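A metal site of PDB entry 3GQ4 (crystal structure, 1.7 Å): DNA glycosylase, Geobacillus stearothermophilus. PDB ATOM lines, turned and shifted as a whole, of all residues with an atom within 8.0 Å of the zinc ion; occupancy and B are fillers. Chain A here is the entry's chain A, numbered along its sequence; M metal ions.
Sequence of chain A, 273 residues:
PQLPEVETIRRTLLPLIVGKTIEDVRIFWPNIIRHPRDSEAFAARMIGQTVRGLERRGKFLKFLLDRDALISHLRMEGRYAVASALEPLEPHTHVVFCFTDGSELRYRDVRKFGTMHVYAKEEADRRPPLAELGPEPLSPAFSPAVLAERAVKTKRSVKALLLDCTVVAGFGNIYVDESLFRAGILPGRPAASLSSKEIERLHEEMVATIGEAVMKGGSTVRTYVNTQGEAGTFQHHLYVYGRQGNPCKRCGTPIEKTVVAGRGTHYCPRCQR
Within 4 Å of the zinc ion: Cys 248, Cys 251, Cys 268 and Cys 271.
The side-chain sulfur (SG) of Cys 248 binds the zinc ion.
SG of Cys 251 is bound to the zinc ion, 2.3 Å away.
SG of Cys 271 binds the zinc ion (2.4 Å).
The zinc ion is bound by the side-chain sulfur (SG) of Cys 268 (2.4 Å).
The zinc ion has four donor atoms within binding distance.
The backbone NH of Cys 248 is in hydrogen-bond range of the backbone carbonyl oxygen of Thr 253.
OG1 of Thr 253 lies close to SG of Cys 251, at 3.1 Å.
N of Cys 268 is in hydrogen-bond range of OE1 of Gln 272, at 2.8 Å.
The side-chain sulfur of Cys 248 sits close to the backbone NH of Arg 250, 3.4 Å away.
SG of Cys 268 lies close to N of Arg 270, 3.4 Å away.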
ATOM      1  N   PHE A 181       0.802  12.443   6.874  1.00  0.00           N
ATOM      2  CA  PHE A 181       1.432  11.185   6.478  1.00  0.00           C
ATOM      3  C   PHE A 181       2.876  11.419   6.022  1.00  0.00           C
ATOM      4  O   PHE A 181       3.809  10.718   6.457  1.00  0.00           O
ATOM      5  CB  PHE A 181       0.655  10.480   5.365  1.00  0.00           C
ATOM      6  CG  PHE A 181       1.431   9.333   4.769  1.00  0.00           C
ATOM      7  CD1 PHE A 181       1.386   8.056   5.348  1.00  0.00           C
ATOM      8  CD2 PHE A 181       2.239   9.543   3.657  1.00  0.00           C
ATOM      9  CE1 PHE A 181       2.112   7.002   4.813  1.00  0.00           C
ATOM     10  CE2 PHE A 181       2.996   8.484   3.111  1.00  0.00           C
ATOM     11  CZ  PHE A 181       2.911   7.214   3.701  1.00  0.00           C
ATOM     12  N   TYR A 239      -1.311   9.453  -0.710  1.00  0.00           N
ATOM     13  CA  TYR A 239      -0.834   8.320   0.073  1.00  0.00           C
ATOM     14  C   TYR A 239      -1.896   7.716   0.990  1.00  0.00           C
ATOM     15  O   TYR A 239      -1.865   6.506   1.295  1.00  0.00           O
ATOM     16  CB  TYR A 239       0.334   8.765   0.940  1.00  0.00           C
ATOM     17  CG  TYR A 239       1.589   9.054   0.186  1.00  0.00           C
ATOM     18  CD1 TYR A 239       2.408   8.018  -0.265  1.00  0.00           C
ATOM     19  CD2 TYR A 239       1.967  10.371  -0.079  1.00  0.00           C
ATOM     20  CE1 TYR A 239       3.568   8.286  -0.961  1.00  0.00           C
ATOM     21  CE2 TYR A 239       3.129  10.644  -0.789  1.00  0.00           C
ATOM     22  CZ  TYR A 239       3.920   9.592  -1.220  1.00  0.00           C
ATOM     23  OH  TYR A 239       5.080   9.864  -1.907  1.00  0.00           O
ATOM     24  N   VAL A 240      -2.802   8.556   1.499  1.00  0.00           N
ATOM     25  CA  VAL A 240      -3.733   8.101   2.539  1.00  0.00           C
ATOM     26  C   VAL A 240      -5.185   8.509   2.328  1.00  0.00           C
ATOM     27  O   VAL A 240      -6.085   7.707   2.590  1.00  0.00           O
ATOM     28  CB  VAL A 240      -3.272   8.521   3.993  1.00  0.00           C
ATOM     29  CG1 VAL A 240      -1.930   7.867   4.364  1.00  0.00           C
ATOM     30  CG2 VAL A 240      -3.187  10.063   4.170  1.00  0.00           C
ATOM     31  N   PRO A 247      -3.229  -0.999   0.852  1.00  0.00           N
ATOM     32  CA  PRO A 247      -1.877  -0.959   1.407  1.00  0.00           C
ATOM     33  C   PRO A 247      -1.243   0.420   1.320  1.00  0.00           C
ATOM     34  O   PRO A 247      -1.386   1.108   0.300  1.00  0.00           O
ATOM     35  CB  PRO A 247      -1.092  -1.949   0.533  1.00  0.00           C
ATOM     36  CG  PRO A 247      -2.113  -2.731  -0.204  1.00  0.00           C
ATOM     37  CD  PRO A 247      -3.321  -1.883  -0.328  1.00  0.00           C
ATOM     38  N   CYS A 248      -0.528   0.806   2.369  1.00  0.00           N
ATOM     39  CA  CYS A 248       0.341   1.972   2.320  1.00  0.00           C
ATOM     40  C   CYS A 248       1.326   1.821   1.162  1.00  0.00           C
ATOM     41  O   CYS A 248       1.907   0.760   0.954  1.00  0.00           O
ATOM     42  CB  CYS A 248       1.106   2.081   3.632  1.00  0.00           C
ATOM     43  SG  CYS A 248       2.244   3.496   3.677  1.00  0.00           S
ATOM     44  N   LYS A 249       1.480   2.892   0.394  1.00  0.00           N
ATOM     45  CA  LYS A 249       2.376   2.899  -0.764  1.00  0.00           C
ATOM     46  C   LYS A 249       3.844   2.766  -0.347  1.00  0.00           C
ATOM     47  O   LYS A 249       4.693   2.372  -1.160  1.00  0.00           O
ATOM     48  CB  LYS A 249       2.178   4.181  -1.563  1.00  0.00           C
ATOM     49  CG  LYS A 249       0.815   4.286  -2.214  1.00  0.00           C
ATOM     50  CD  LYS A 249       0.717   5.524  -3.109  1.00  0.00           C
ATOM     51  CE  LYS A 249      -0.619   5.603  -3.794  1.00  0.00           C
ATOM     52  NZ  LYS A 249      -0.674   6.762  -4.754  1.00  0.00           N
ATOM     53  N   ARG A 250       4.123   3.091   0.918  1.00  0.00           N
ATOM     54  CA  ARG A 250       5.500   3.057   1.406  1.00  0.00           C
ATOM     55  C   ARG A 250       5.857   1.810   2.202  1.00  0.00           C
ATOM     56  O   ARG A 250       6.985   1.322   2.095  1.00  0.00           O
ATOM     57  CB  ARG A 250       5.815   4.319   2.198  1.00  0.00           C
ATOM     58  CG  ARG A 250       5.519   5.589   1.399  1.00  0.00           C
ATOM     59  CD  ARG A 250       6.674   6.571   1.394  1.00  0.00           C
ATOM     60  NE  ARG A 250       6.571   7.543   2.469  1.00  0.00           N
ATOM     61  CZ  ARG A 250       6.787   8.851   2.337  1.00  0.00           C
ATOM     62  NH1 ARG A 250       6.669   9.632   3.388  1.00  0.00           N
ATOM     63  NH2 ARG A 250       7.110   9.372   1.158  1.00  0.00           N
ATOM     64  N   CYS A 251       4.916   1.293   2.997  1.00  0.00           N
ATOM     65  CA  CYS A 251       5.246   0.157   3.888  1.00  0.00           C
ATOM     66  C   CYS A 251       4.282  -1.026   3.753  1.00  0.00           C
ATOM     67  O   CYS A 251       4.521  -2.095   4.346  1.00  0.00           O
ATOM     68  CB  CYS A 251       5.296   0.607   5.351  1.00  0.00           C
ATOM     69  SG  CYS A 251       3.659   0.902   6.054  1.00  0.00           S
ATOM     70  N   GLY A 252       3.215  -0.847   2.987  1.00  0.00           N
ATOM     71  CA  GLY A 252       2.255  -1.941   2.746  1.00  0.00           C
ATOM     72  C   GLY A 252       1.237  -2.189   3.842  1.00  0.00           C
ATOM     73  O   GLY A 252       0.349  -3.032   3.673  1.00  0.00           O
ATOM     74  N   THR A 253       1.353  -1.474   4.976  1.00  0.00           N
ATOM     75  CA  THR A 253       0.386  -1.625   6.070  1.00  0.00           C
ATOM     76  C   THR A 253      -0.958  -1.036   5.608  1.00  0.00           C
ATOM     77  O   THR A 253      -0.957   0.014   4.956  1.00  0.00           O
ATOM     78  CB  THR A 253       0.879  -0.853   7.311  1.00  0.00           C
ATOM     79  OG1 THR A 253       2.186  -1.322   7.656  1.00  0.00           O
ATOM     80  CG2 THR A 253      -0.067  -1.036   8.528  1.00  0.00           C
ATOM     81  N   PRO A 254      -2.082  -1.693   5.939  1.00  0.00           N
ATOM     82  CA  PRO A 254      -3.371  -1.127   5.494  1.00  0.00           C
ATOM     83  C   PRO A 254      -3.621   0.258   6.077  1.00  0.00           C
ATOM     84  O   PRO A 254      -3.418   0.493   7.287  1.00  0.00           O
ATOM     85  CB  PRO A 254      -4.411  -2.138   6.021  1.00  0.00           C
ATOM     86  CG  PRO A 254      -3.649  -3.428   6.080  1.00  0.00           C
ATOM     87  CD  PRO A 254      -2.251  -3.023   6.559  1.00  0.00           C
ATOM     88  N   ILE A 255      -4.030   1.182   5.218  1.00  0.00           N
ATOM     89  CA  ILE A 255      -4.398   2.517   5.654  1.00  0.00           C
ATOM     90  C   ILE A 255      -5.675   2.422   6.510  1.00  0.00           C
ATOM     91  O   ILE A 255      -6.588   1.634   6.219  1.00  0.00           O
ATOM     92  CB  ILE A 255      -4.585   3.453   4.439  1.00  0.00           C
ATOM     93  CG1 ILE A 255      -3.270   3.548   3.635  1.00  0.00           C
ATOM     94  CG2 ILE A 255      -5.115   4.834   4.852  1.00  0.00           C
ATOM     95  CD1 ILE A 255      -2.001   3.944   4.497  1.00  0.00           C
ATOM     96  N   TYR A 267      -4.800   7.547   7.760  1.00  0.00           N
ATOM     97  CA  TYR A 267      -3.416   7.523   8.200  1.00  0.00           C
ATOM     98  C   TYR A 267      -2.808   6.123   8.054  1.00  0.00           C
ATOM     99  O   TYR A 267      -3.545   5.128   8.021  1.00  0.00           O
ATOM    100  CB  TYR A 267      -3.303   8.010   9.665  1.00  0.00           C
ATOM    101  CG  TYR A 267      -4.061   7.106  10.611  1.00  0.00           C
ATOM    102  CD1 TYR A 267      -3.410   6.107  11.314  1.00  0.00           C
ATOM    103  CD2 TYR A 267      -5.444   7.262  10.781  1.00  0.00           C
ATOM    104  CE1 TYR A 267      -4.115   5.247  12.172  1.00  0.00           C
ATOM    105  CE2 TYR A 267      -6.166   6.416  11.633  1.00  0.00           C
ATOM    106  CZ  TYR A 267      -5.484   5.413  12.325  1.00  0.00           C
ATOM    107  OH  TYR A 267      -6.187   4.586  13.157  1.00  0.00           O
ATOM    108  N   CYS A 268      -1.491   6.056   8.001  1.00  0.00           N
ATOM    109  CA  CYS A 268      -0.792   4.787   8.132  1.00  0.00           C
ATOM    110  C   CYS A 268      -0.286   4.636   9.562  1.00  0.00           C
ATOM    111  O   CYS A 268       0.503   5.472  10.014  1.00  0.00           O
ATOM    112  CB  CYS A 268       0.390   4.720   7.178  1.00  0.00           C
ATOM    113  SG  CYS A 268       1.314   3.189   7.412  1.00  0.00           S
ATOM    114  N   PRO A 269      -0.705   3.575  10.275  1.00  0.00           N
ATOM    115  CA  PRO A 269      -0.321   3.459  11.663  1.00  0.00           C
ATOM    116  C   PRO A 269       1.133   3.052  11.852  1.00  0.00           C
ATOM    117  O   PRO A 269       1.629   3.056  12.985  1.00  0.00           O
ATOM    118  CB  PRO A 269      -1.251   2.362  12.189  1.00  0.00           C
ATOM    119  CG  PRO A 269      -1.497   1.521  11.009  1.00  0.00           C
ATOM    120  CD  PRO A 269      -1.598   2.479   9.856  1.00  0.00           C
ATOM    121  N   ARG A 270       1.813   2.682  10.764  1.00  0.00           N
ATOM    122  CA  ARG A 270       3.245   2.405  10.820  1.00  0.00           C
ATOM    123  C   ARG A 270       4.129   3.609  10.490  1.00  0.00           C
ATOM    124  O   ARG A 270       5.078   3.922  11.231  1.00  0.00           O
ATOM    125  CB  ARG A 270       3.606   1.224   9.911  1.00  0.00           C
ATOM    126  CG  ARG A 270       5.097   0.894   9.944  1.00  0.00           C
ATOM    127  CD  ARG A 270       5.400  -0.346   9.141  1.00  0.00           C
ATOM    128  NE  ARG A 270       6.807  -0.688   9.260  1.00  0.00           N
ATOM    129  CZ  ARG A 270       7.338  -1.851   8.893  1.00  0.00           C
ATOM    130  NH1 ARG A 270       8.625  -2.053   9.077  1.00  0.00           N
ATOM    131  NH2 ARG A 270       6.580  -2.814   8.364  1.00  0.00           N
ATOM    132  N   CYS A 271       3.819   4.277   9.378  1.00  0.00           N
ATOM    133  CA  CYS A 271       4.622   5.424   8.914  1.00  0.00           C
ATOM    134  C   CYS A 271       4.431   6.639   9.799  1.00  0.00           C
ATOM    135  O   CYS A 271       5.331   7.497   9.884  1.00  0.00           O
ATOM    136  CB  CYS A 271       4.265   5.782   7.471  1.00  0.00           C
ATOM    137  SG  CYS A 271       4.867   4.586   6.260  1.00  0.00           S
ATOM    138  N   GLN A 272       3.284   6.735  10.442  1.00  0.00           N
ATOM    139  CA  GLN A 272       2.973   7.919  11.270  1.00  0.00           C
ATOM    140  C   GLN A 272       3.053   7.559  12.751  1.00  0.00           C
ATOM    141  O   GLN A 272       2.603   6.490  13.173  1.00  0.00           O
ATOM    142  CB  GLN A 272       1.592   8.478  10.889  1.00  0.00           C
ATOM    143  CG  GLN A 272       1.573   9.055   9.474  1.00  0.00           C
ATOM    144  CD  GLN A 272       0.176   9.362   8.986  1.00  0.00           C
ATOM    145  OE1 GLN A 272      -0.401   8.611   8.200  1.00  0.00           O
ATOM    146  NE2 GLN A 272      -0.392  10.499   9.444  1.00  0.00           N
HETATM  147 ZN    ZN M   1       3.059   3.143   5.826  1.00  0.00          ZN
